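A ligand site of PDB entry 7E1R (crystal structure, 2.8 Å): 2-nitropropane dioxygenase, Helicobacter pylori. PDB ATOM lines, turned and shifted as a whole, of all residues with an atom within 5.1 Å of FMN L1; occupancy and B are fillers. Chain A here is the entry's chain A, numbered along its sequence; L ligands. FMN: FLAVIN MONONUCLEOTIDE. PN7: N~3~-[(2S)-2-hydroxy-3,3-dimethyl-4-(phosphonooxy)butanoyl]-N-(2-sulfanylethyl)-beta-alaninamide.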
ATOM      1  N   GLY A  31       7.631 -24.590  -3.065  1.00  0.00           N
ATOM      2  CA  GLY A  31       6.729 -23.863  -3.945  1.00  0.00           C
ATOM      3  C   GLY A  31       5.524 -23.297  -3.200  1.00  0.00           C
ATOM      4  O   GLY A  31       4.974 -23.921  -2.290  1.00  0.00           O
ATOM      5  N   GLY A  32       5.111 -22.099  -3.608  1.00  0.00           N
ATOM      6  CA  GLY A  32       3.936 -21.496  -3.014  1.00  0.00           C
ATOM      7  C   GLY A  32       2.701 -22.345  -3.253  1.00  0.00           C
ATOM      8  O   GLY A  32       2.509 -22.900  -4.334  1.00  0.00           O
ATOM      9  N   MET A  33       1.849 -22.459  -2.224  1.00  0.00           N
ATOM     10  CA  MET A  33       0.633 -23.268  -2.318  1.00  0.00           C
ATOM     11  C   MET A  33      -0.525 -22.396  -1.836  1.00  0.00           C
ATOM     12  O   MET A  33      -0.612 -22.040  -0.655  1.00  0.00           O
ATOM     13  CB  MET A  33       0.805 -24.579  -1.543  1.00  0.00           C
ATOM     14  CG  MET A  33       1.746 -25.516  -2.302  1.00  0.00           C
ATOM     15  SD  MET A  33       2.095 -27.166  -1.653  1.00  0.00           S
ATOM     16  CE  MET A  33       3.121 -26.818  -0.236  1.00  0.00           C
ATOM     17  N   GLY A  34      -1.417 -22.106  -2.787  1.00  0.00           N
ATOM     18  CA  GLY A  34      -2.496 -21.156  -2.568  1.00  0.00           C
ATOM     19  C   GLY A  34      -3.642 -21.503  -1.633  1.00  0.00           C
ATOM     20  O   GLY A  34      -4.176 -22.615  -1.610  1.00  0.00           O
ATOM     21  N   ILE A  37      -2.036 -23.073   2.532  1.00  0.00           N
ATOM     22  CA  ILE A  37      -1.251 -24.296   2.621  1.00  0.00           C
ATOM     23  C   ILE A  37       0.161 -23.975   3.054  1.00  0.00           C
ATOM     24  O   ILE A  37       0.687 -24.595   3.966  1.00  0.00           O
ATOM     25  CB  ILE A  37      -1.347 -25.049   1.288  1.00  0.00           C
ATOM     26  CG1 ILE A  37      -2.817 -25.312   1.052  1.00  0.00           C
ATOM     27  CG2 ILE A  37      -1.064 -26.379   1.452  1.00  0.00           C
ATOM     28  CD1 ILE A  37      -3.146 -25.811  -0.313  1.00  0.00           C
ATOM     29  N   SER A  56       2.319 -18.118   0.232  1.00  0.00           N
ATOM     30  CA  SER A  56       1.284 -17.813  -0.752  1.00  0.00           C
ATOM     31  C   SER A  56       0.484 -16.601  -0.284  1.00  0.00           C
ATOM     32  O   SER A  56      -0.058 -16.584   0.815  1.00  0.00           O
ATOM     33  CB  SER A  56       0.354 -19.001  -0.966  1.00  0.00           C
ATOM     34  OG  SER A  56      -0.722 -18.633  -1.810  1.00  0.00           O
ATOM     35  N   VAL A  58      -2.235 -15.555  -1.736  1.00  0.00           N
ATOM     36  CA  VAL A  58      -3.581 -15.664  -2.286  1.00  0.00           C
ATOM     37  C   VAL A  58      -4.532 -16.060  -1.159  1.00  0.00           C
ATOM     38  O   VAL A  58      -4.285 -17.029  -0.428  1.00  0.00           O
ATOM     39  CB  VAL A  58      -3.608 -16.695  -3.422  1.00  0.00           C
ATOM     40  CG1 VAL A  58      -5.028 -17.023  -3.819  1.00  0.00           C
ATOM     41  CG2 VAL A  58      -2.809 -16.187  -4.601  1.00  0.00           C
ATOM     42  N   ASN A 108       4.320 -15.795  -3.128  1.00  0.00           N
ATOM     43  CA  ASN A 108       3.780 -16.290  -4.400  1.00  0.00           C
ATOM     44  C   ASN A 108       2.448 -15.592  -4.695  1.00  0.00           C
ATOM     45  O   ASN A 108       1.526 -15.616  -3.882  1.00  0.00           O
ATOM     46  CB  ASN A 108       3.602 -17.815  -4.370  1.00  0.00           C
ATOM     47  CG  ASN A 108       3.067 -18.361  -5.672  1.00  0.00           C
ATOM     48  OD1 ASN A 108       1.889 -18.200  -6.006  1.00  0.00           O
ATOM     49  ND2 ASN A 108       3.948 -19.006  -6.437  1.00  0.00           N
ATOM     50  N   LEU A 110      -0.294 -15.223  -7.930  1.00  0.00           N
ATOM     51  CA  LEU A 110      -0.733 -15.528  -9.286  1.00  0.00           C
ATOM     52  C   LEU A 110      -0.988 -14.239 -10.058  1.00  0.00           C
ATOM     53  O   LEU A 110      -1.607 -13.307  -9.548  1.00  0.00           O
ATOM     54  CB  LEU A 110      -2.030 -16.336  -9.239  1.00  0.00           C
ATOM     55  CG  LEU A 110      -2.078 -17.858  -9.083  1.00  0.00           C
ATOM     56  CD1 LEU A 110      -1.728 -18.284  -7.659  1.00  0.00           C
ATOM     57  CD2 LEU A 110      -3.462 -18.340  -9.472  1.00  0.00           C
ATOM     58  N   GLY A 134       3.368 -16.876 -11.321  1.00  0.00           N
ATOM     59  CA  GLY A 134       2.971 -17.672 -12.468  1.00  0.00           C
ATOM     60  C   GLY A 134       1.558 -17.343 -12.904  1.00  0.00           C
ATOM     61  O   GLY A 134       1.089 -16.216 -12.722  1.00  0.00           O
ATOM     62  N   ILE A 156       7.297 -17.454 -13.489  1.00  0.00           N
ATOM     63  CA  ILE A 156       7.132 -18.865 -13.803  1.00  0.00           C
ATOM     64  C   ILE A 156       6.749 -18.975 -15.270  1.00  0.00           C
ATOM     65  O   ILE A 156       5.832 -18.287 -15.740  1.00  0.00           O
ATOM     66  CB  ILE A 156       6.058 -19.524 -12.930  1.00  0.00           C
ATOM     67  CG1 ILE A 156       6.371 -19.318 -11.452  1.00  0.00           C
ATOM     68  CG2 ILE A 156       5.998 -21.006 -13.228  1.00  0.00           C
ATOM     69  CD1 ILE A 156       5.414 -20.045 -10.536  1.00  0.00           C
ATOM     70  N   GLU A 184       8.117 -24.468 -14.934  1.00  0.00           N
ATOM     71  CA  GLU A 184       7.183 -25.393 -14.291  1.00  0.00           C
ATOM     72  C   GLU A 184       6.632 -26.418 -15.278  1.00  0.00           C
ATOM     73  O   GLU A 184       5.929 -26.045 -16.223  1.00  0.00           O
ATOM     74  CB  GLU A 184       6.015 -24.699 -13.603  1.00  0.00           C
ATOM     75  CG  GLU A 184       5.352 -25.649 -12.634  1.00  0.00           C
ATOM     76  CD  GLU A 184       4.141 -25.073 -11.942  1.00  0.00           C
ATOM     77  OE1 GLU A 184       3.395 -24.292 -12.578  1.00  0.00           O
ATOM     78  OE2 GLU A 184       3.983 -25.401 -10.736  1.00  0.00           O
ATOM     79  N   LEU A 187       3.723 -31.728 -14.395  1.00  0.00           N
ATOM     80  CA  LEU A 187       3.341 -32.621 -13.336  1.00  0.00           C
ATOM     81  C   LEU A 187       3.161 -31.902 -12.056  1.00  0.00           C
ATOM     82  O   LEU A 187       2.954 -32.492 -11.085  1.00  0.00           O
ATOM     83  CB  LEU A 187       4.359 -33.676 -13.133  1.00  0.00           C
ATOM     84  CG  LEU A 187       5.144 -34.232 -14.259  1.00  0.00           C
ATOM     85  CD1 LEU A 187       6.183 -33.223 -14.698  1.00  0.00           C
ATOM     86  CD2 LEU A 187       5.799 -35.422 -13.653  1.00  0.00           C
ATOM     87  N   SER A 188       3.079 -30.626 -12.093  1.00  0.00           N
ATOM     88  CA  SER A 188       2.933 -29.839 -10.944  1.00  0.00           C
ATOM     89  C   SER A 188       1.564 -29.717 -10.382  1.00  0.00           C
ATOM     90  O   SER A 188       0.611 -30.037 -11.019  1.00  0.00           O
ATOM     91  CB  SER A 188       3.465 -28.489 -11.265  1.00  0.00           C
ATOM     92  OG  SER A 188       2.967 -27.973 -12.451  1.00  0.00           O
ATOM     93  N   GLY A 189       1.462 -29.260  -9.153  1.00  0.00           N
ATOM     94  CA  GLY A 189       0.152 -29.119  -8.573  1.00  0.00           C
ATOM     95  C   GLY A 189      -0.479 -27.790  -8.956  1.00  0.00           C
ATOM     96  O   GLY A 189       0.186 -26.880  -9.453  1.00  0.00           O
ATOM     97  N   GLY A 190      -1.788 -27.665  -8.761  1.00  0.00           N
ATOM     98  CA  GLY A 190      -2.398 -26.383  -9.033  1.00  0.00           C
ATOM     99  C   GLY A 190      -2.503 -26.197 -10.534  1.00  0.00           C
ATOM    100  O   GLY A 190      -2.648 -27.153 -11.289  1.00  0.00           O
ATOM    101  N   ALA A 228      10.757 -27.052 -11.857  1.00  0.00           N
ATOM    102  CA  ALA A 228       9.682 -27.427 -10.947  1.00  0.00           C
ATOM    103  C   ALA A 228       8.710 -28.368 -11.636  1.00  0.00           C
ATOM    104  O   ALA A 228       8.467 -28.247 -12.839  1.00  0.00           O
ATOM    105  CB  ALA A 228       8.929 -26.184 -10.448  1.00  0.00           C
ATOM    106  N   GLY A 229       8.175 -29.309 -10.869  1.00  0.00           N
ATOM    107  CA  GLY A 229       7.103 -30.167 -11.328  1.00  0.00           C
ATOM    108  C   GLY A 229       7.462 -31.635 -11.418  1.00  0.00           C
ATOM    109  O   GLY A 229       8.078 -32.081 -12.391  1.00  0.00           O
ATOM    110  N   GLY A 230       7.113 -32.398 -10.383  1.00  0.00           N
ATOM    111  CA  GLY A 230       7.414 -33.812 -10.355  1.00  0.00           C
ATOM    112  C   GLY A 230       8.700 -34.184  -9.675  1.00  0.00           C
ATOM    113  O   GLY A 230       9.036 -35.375  -9.615  1.00  0.00           O
ATOM    114  N   ILE A 231       9.420 -33.219  -9.110  1.00  0.00           N
ATOM    115  CA  ILE A 231      10.699 -33.509  -8.486  1.00  0.00           C
ATOM    116  C   ILE A 231      10.444 -34.066  -7.094  1.00  0.00           C
ATOM    117  O   ILE A 231       9.851 -33.385  -6.249  1.00  0.00           O
ATOM    118  CB  ILE A 231      11.569 -32.240  -8.422  1.00  0.00           C
ATOM    119  CG1 ILE A 231      11.864 -31.753  -9.837  1.00  0.00           C
ATOM    120  CG2 ILE A 231      12.825 -32.522  -7.646  1.00  0.00           C
ATOM    121  CD1 ILE A 231      12.310 -30.322  -9.910  1.00  0.00           C
ATOM    122  N   GLN A 249      12.244 -26.291  -7.490  1.00  0.00           N
ATOM    123  CA  GLN A 249      11.109 -25.911  -6.665  1.00  0.00           C
ATOM    124  C   GLN A 249      10.217 -27.131  -6.494  1.00  0.00           C
ATOM    125  O   GLN A 249       9.802 -27.760  -7.479  1.00  0.00           O
ATOM    126  CB  GLN A 249      10.315 -24.767  -7.294  1.00  0.00           C
ATOM    127  CG  GLN A 249       8.976 -24.457  -6.602  1.00  0.00           C
ATOM    128  CD  GLN A 249       8.324 -23.175  -7.081  1.00  0.00           C
ATOM    129  OE1 GLN A 249       8.615 -22.073  -6.595  1.00  0.00           O
ATOM    130  NE2 GLN A 249       7.414 -23.295  -8.043  1.00  0.00           N
ATOM    131  N   MET A 250       9.936 -27.463  -5.237  1.00  0.00           N
ATOM    132  CA  MET A 250       9.093 -28.586  -4.884  1.00  0.00           C
ATOM    133  C   MET A 250       7.924 -28.111  -4.025  1.00  0.00           C
ATOM    134  O   MET A 250       8.054 -27.162  -3.247  1.00  0.00           O
ATOM    135  CB  MET A 250       9.898 -29.634  -4.140  1.00  0.00           C
ATOM    136  CG  MET A 250      11.041 -30.176  -4.959  1.00  0.00           C
ATOM    137  SD  MET A 250      11.956 -31.385  -3.998  1.00  0.00           S
ATOM    138  CE  MET A 250      13.476 -30.484  -3.781  1.00  0.00           C
ATOM    139  N   ALA A 251       6.801 -28.820  -4.123  1.00  0.00           N
ATOM    140  CA  ALA A 251       5.648 -28.418  -3.337  1.00  0.00           C
ATOM    141  C   ALA A 251       4.945 -29.622  -2.731  1.00  0.00           C
ATOM    142  O   ALA A 251       4.664 -29.629  -1.528  1.00  0.00           O
ATOM    143  CB  ALA A 251       4.675 -27.619  -4.204  1.00  0.00           C
ATOM    144  N   THR A 252       4.658 -30.651  -3.555  1.00  0.00           N
ATOM    145  CA  THR A 252       3.959 -31.836  -3.062  1.00  0.00           C
ATOM    146  C   THR A 252       4.648 -32.461  -1.851  1.00  0.00           C
ATOM    147  O   THR A 252       3.998 -32.808  -0.856  1.00  0.00           O
ATOM    148  CB  THR A 252       3.814 -32.854  -4.190  1.00  0.00           C
ATOM    149  OG1 THR A 252       3.013 -32.297  -5.234  1.00  0.00           O
ATOM    150  CG2 THR A 252       3.134 -34.103  -3.671  1.00  0.00           C
ATOM    151  N   LEU A 255       3.807 -30.323   0.878  1.00  0.00           N
ATOM    152  CA  LEU A 255       2.408 -30.600   1.166  1.00  0.00           C
ATOM    153  C   LEU A 255       2.279 -31.809   2.086  1.00  0.00           C
ATOM    154  O   LEU A 255       1.312 -31.911   2.848  1.00  0.00           O
ATOM    155  CB  LEU A 255       1.640 -30.809  -0.141  1.00  0.00           C
ATOM    156  CG  LEU A 255       0.121 -30.890  -0.090  1.00  0.00           C
ATOM    157  CD1 LEU A 255      -0.458 -29.588   0.423  1.00  0.00           C
ATOM    158  CD2 LEU A 255      -0.453 -31.233  -1.473  1.00  0.00           C
ATOM    159  N   TYR A 265      -4.645 -31.602   4.938  1.00  0.00           N
ATOM    160  CA  TYR A 265      -3.848 -32.428   4.037  1.00  0.00           C
ATOM    161  C   TYR A 265      -3.106 -33.531   4.760  1.00  0.00           C
ATOM    162  O   TYR A 265      -2.952 -34.625   4.201  1.00  0.00           O
ATOM    163  CB  TYR A 265      -2.836 -31.607   3.238  1.00  0.00           C
ATOM    164  CG  TYR A 265      -3.400 -30.892   2.047  1.00  0.00           C
ATOM    165  CD1 TYR A 265      -3.472 -31.545   0.829  1.00  0.00           C
ATOM    166  CD2 TYR A 265      -3.899 -29.608   2.138  1.00  0.00           C
ATOM    167  CE1 TYR A 265      -3.984 -30.943  -0.278  1.00  0.00           C
ATOM    168  CE2 TYR A 265      -4.428 -28.974   1.022  1.00  0.00           C
ATOM    169  CZ  TYR A 265      -4.475 -29.662  -0.182  1.00  0.00           C
ATOM    170  OH  TYR A 265      -4.984 -29.082  -1.312  1.00  0.00           O
ATOM    171  N   PHE A 348      -5.815 -29.599  -3.991  1.00  0.00           N
ATOM    172  CA  PHE A 348      -4.853 -29.687  -5.083  1.00  0.00           C
ATOM    173  C   PHE A 348      -3.742 -30.661  -4.702  1.00  0.00           C
ATOM    174  O   PHE A 348      -3.507 -30.947  -3.531  1.00  0.00           O
ATOM    175  CB  PHE A 348      -4.252 -28.319  -5.406  1.00  0.00           C
ATOM    176  CG  PHE A 348      -5.133 -27.442  -6.244  1.00  0.00           C
ATOM    177  CD1 PHE A 348      -6.235 -27.960  -6.899  1.00  0.00           C
ATOM    178  CD2 PHE A 348      -4.836 -26.102  -6.413  1.00  0.00           C
ATOM    179  CE1 PHE A 348      -7.045 -27.155  -7.679  1.00  0.00           C
ATOM    180  CE2 PHE A 348      -5.637 -25.277  -7.191  1.00  0.00           C
ATOM    181  CZ  PHE A 348      -6.745 -25.806  -7.818  1.00  0.00           C
ATOM    182  N   THR A 349      -3.017 -31.114  -5.712  1.00  0.00           N
ATOM    183  CA  THR A 349      -1.857 -31.969  -5.496  1.00  0.00           C
ATOM    184  C   THR A 349      -1.024 -32.028  -6.764  1.00  0.00           C
ATOM    185  O   THR A 349      -1.529 -31.847  -7.869  1.00  0.00           O
ATOM    186  CB  THR A 349      -2.216 -33.391  -5.081  1.00  0.00           C
ATOM    187  OG1 THR A 349      -1.013 -34.150  -4.869  1.00  0.00           O
ATOM    188  CG2 THR A 349      -3.020 -34.056  -6.183  1.00  0.00           C
ATOM    189  N   GLY A 350       0.262 -32.296  -6.577  1.00  0.00           N
ATOM    190  CA  GLY A 350       1.091 -32.699  -7.679  1.00  0.00           C
ATOM    191  C   GLY A 350       0.760 -34.121  -8.101  1.00  0.00           C
ATOM    192  O   GLY A 350       0.115 -34.880  -7.388  1.00  0.00           O
ATOM    193  N   ALA A 351       1.287 -34.498  -9.272  1.00  0.00           N
ATOM    194  CA  ALA A 351       1.067 -35.855  -9.768  1.00  0.00           C
ATOM    195  C   ALA A 351       1.671 -36.910  -8.841  1.00  0.00           C
ATOM    196  O   ALA A 351       1.189 -38.042  -8.817  1.00  0.00           O
ATOM    197  CB  ALA A 351       1.655 -35.998 -11.172  1.00  0.00           C
ATOM    198  N   ASN A 352       2.682 -36.553  -8.069  1.00  0.00           N
ATOM    199  CA  ASN A 352       3.279 -37.501  -7.130  1.00  0.00           C
ATOM    200  C   ASN A 352       2.569 -37.578  -5.794  1.00  0.00           C
ATOM    201  O   ASN A 352       3.059 -38.265  -4.891  1.00  0.00           O
ATOM    202  CB  ASN A 352       4.758 -37.166  -6.918  1.00  0.00           C
ATOM    203  CG  ASN A 352       5.597 -37.453  -8.158  1.00  0.00           C
ATOM    204  OD1 ASN A 352       5.340 -38.422  -8.866  1.00  0.00           O
ATOM    205  ND2 ASN A 352       6.585 -36.608  -8.421  1.00  0.00           N
HETATM  206  N1  FMN L   1       1.899 -22.510  -7.728  1.00  0.00           N
HETATM  207  C2  FMN L   1       1.732 -21.127  -7.717  1.00  0.00           C
HETATM  208  O2  FMN L   1       2.459 -20.414  -8.419  1.00  0.00           O
HETATM  209  N3  FMN L   1       0.739 -20.536  -6.918  1.00  0.00           N
HETATM  210  C4  FMN L   1      -0.074 -21.349  -6.129  1.00  0.00           C
HETATM  211  O4  FMN L   1      -0.940 -20.821  -5.426  1.00  0.00           O
HETATM  212  C4A FMN L   1       0.082 -22.741  -6.150  1.00  0.00           C
HETATM  213  N5  FMN L   1      -0.702 -23.521  -5.393  1.00  0.00           N
HETATM  214  C5A FMN L   1      -0.420 -24.833  -5.284  1.00  0.00           C
HETATM  215  C6  FMN L   1      -1.137 -25.607  -4.362  1.00  0.00           C
HETATM  216  C7  FMN L   1      -0.853 -26.961  -4.196  1.00  0.00           C
HETATM  217  C7M FMN L   1      -1.576 -27.702  -3.259  1.00  0.00           C
HETATM  218  C8  FMN L   1       0.150 -27.545  -4.961  1.00  0.00           C
HETATM  219  C8M FMN L   1       0.453 -28.901  -4.835  1.00  0.00           C
HETATM  220  C9  FMN L   1       0.846 -26.772  -5.888  1.00  0.00           C
HETATM  221  C9A FMN L   1       0.575 -25.414  -6.052  1.00  0.00           C
HETATM  222  N10 FMN L   1       1.257 -24.655  -6.941  1.00  0.00           N
HETATM  223  C10 FMN L   1       1.073 -23.327  -6.940  1.00  0.00           C
HETATM  224  C1' FMN L   1       2.449 -25.184  -7.673  1.00  0.00           C
HETATM  225  C2' FMN L   1       3.667 -25.286  -6.735  1.00  0.00           C
HETATM  226  O2' FMN L   1       4.031 -24.002  -6.232  1.00  0.00           O
HETATM  227  C3' FMN L   1       4.891 -25.953  -7.387  1.00  0.00           C
HETATM  228  O3' FMN L   1       5.407 -25.108  -8.422  1.00  0.00           O
HETATM  229  C4' FMN L   1       4.616 -27.335  -8.012  1.00  0.00           C
HETATM  230  O4' FMN L   1       3.552 -27.996  -7.333  1.00  0.00           O
HETATM  231  C5' FMN L   1       5.890 -28.186  -7.931  1.00  0.00           C
HETATM  232  O5' FMN L   1       5.621 -29.535  -8.317  1.00  0.00           O
HETATM  233  P   FMN L   1       5.555 -30.708  -7.226  1.00  0.00           P
HETATM  234  O1P FMN L   1       6.848 -30.545  -6.545  1.00  0.00           O
HETATM  235  O2P FMN L   1       4.368 -30.395  -6.402  1.00  0.00           O
HETATM  236  O3P FMN L   1       5.464 -31.924  -8.029  1.00  0.00           O
HETATM  237  O3  PN7 L   2       3.342 -18.287 -19.330  1.00  0.00           O
HETATM  238  O4  PN7 L   2       0.788 -20.465 -18.550  1.00  0.00           O
HETATM  239  C2  PN7 L   2       1.591 -18.794 -20.924  1.00  0.00           C
HETATM  240  C1  PN7 L   2       0.185 -18.375 -21.440  1.00  0.00           C
HETATM  241  P   PN7 L   2      -1.040 -17.875 -23.941  1.00  0.00           P
HETATM  242  O1P PN7 L   2      -1.319 -16.414 -23.630  1.00  0.00           O
HETATM  243  O2P PN7 L   2      -2.240 -18.795 -23.973  1.00  0.00           O
HETATM  244  O3P PN7 L   2       0.081 -18.494 -22.898  1.00  0.00           O
HETATM  245  CE1 PN7 L   2       1.917 -20.208 -21.364  1.00  0.00           C
HETATM  246  CE2 PN7 L   2       2.567 -17.867 -21.626  1.00  0.00           C
HETATM  247  C3  PN7 L   2       1.930 -18.564 -19.404  1.00  0.00           C
HETATM  248  C4  PN7 L   2       1.727 -19.692 -18.384  1.00  0.00           C
HETATM  249  N5  PN7 L   2       2.532 -19.788 -17.279  1.00  0.00           N
HETATM  250  C6  PN7 L   2       2.488 -20.840 -16.222  1.00  0.00           C
HETATM  251  C7  PN7 L   2       2.085 -20.409 -14.792  1.00  0.00           C
HETATM  252  C8  PN7 L   2       2.051 -21.650 -13.900  1.00  0.00           C
HETATM  253  O8  PN7 L   2       2.691 -22.594 -14.341  1.00  0.00           O
HETATM  254  N9  PN7 L   2       1.404 -21.831 -12.713  1.00  0.00           N
HETATM  255  C10 PN7 L   2       0.530 -21.123 -11.760  1.00  0.00           C
HETATM  256  C11 PN7 L   2       0.345 -22.102 -10.569  1.00  0.00           C
HETATM  257  S12 PN7 L   2      -1.236 -22.112  -9.645  1.00  0.00           S
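The side-chain hydroxyl of Thr 252 sits at hydrogen-bond distance from the backbone NH of Gly 350 (3.1 Å).
OE2 of Glu 184 lies close to OG of Ser 188 (3.3 Å).
The backbone carbonyl oxygen of Gly 230 is in hydrogen-bond range of the side-chain amide nitrogen of Asn 352.
The backbone carbonyl oxygen (O) of Met 250 lies within hydrogen-bond range of the backbone NH (N) of Gly 31 (2.6 Å).
The backbone NH of Phe 348 is in hydrogen-bond range of the side-chain hydroxyl of Tyr 265, 2.9 Å away.
O of Leu 187 is in hydrogen-bond range of N of Ala 351 (3.2 Å).
Gly 31 touches FMN L1.
CA of Met 33 touches N5 of FMN L1, at 3.4 Å.
CD1 of Ile 37 touches C7M of FMN L1, 3.8 Å away.
Leu 110 touches FMN L1.
Ile 156 touches FMN L1 (CD1 to O2, 3.7 Å).
Leu 187 touches FMN L1.
Ser 188 touches FMN L1 (CB to C4', 3.6 Å).
Gly 190 touches FMN L1.
Gly 229 touches FMN L1 (CA to O5', 3.4 Å).
Met 250 touches FMN L1.
CB of Phe 348 touches C7M of FMN L1, at 3.5 Å.
Thr 349 touches FMN L1 (CA to C8M, 3.9 Å).
N of Gly 350 touches C8M of FMN L1, at 3.8 Å.
Hydrophobic or aromatic side chains that line FMN L1: Met 33, Ile 37, Leu 110, Ile 156, Met 250, Ala 251 and Phe 348.
An oxygen (O2P) of FMN L1 sits at hydrogen-bond distance from the backbone NH (N) of Thr 252.
The side-chain hydroxyl (OG1) of Thr 252 sits at hydrogen-bond distance from an oxygen (O2P) of FMN L1.
N of Gly 32 sits at hydrogen-bond distance from O2' of FMN L1 (3.4 Å).
An oxygen (O2') of FMN L1 sits at hydrogen-bond distance from the backbone carbonyl oxygen of Gly 32 (2.7 Å).
The side-chain amide nitrogen (NE2) of Gln 249 is in hydrogen-bond range of an oxygen (O3') of FMN L1.
An oxygen (O3') of FMN L1 sits at hydrogen-bond distance from the side-chain carboxylate of Glu 184 (2.7 Å).
OD1 of Asn 108 lies within hydrogen-bond range of N3 of FMN L1 (2.8 Å).
The backbone NH (N) of Gly 230 lies within hydrogen-bond range of an oxygen (O3P) of FMN L1.
An oxygen (O4) of FMN L1 is in hydrogen-bond range of the backbone NH of Gly 34 (3.0 Å).
N of Ala 251 lies within hydrogen-bond range of O1P of FMN L1.
O4' of FMN L1 is in hydrogen-bond range of N of Gly 189.
A nitrogen (N9) of PN7 L2 lies within hydrogen-bond range of the side-chain carboxylate (OE1) of Glu 184, 3.2 Å away.
A nitrogen (N1) of FMN L1 sits close to a sulfur (S12) of PN7 L2.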
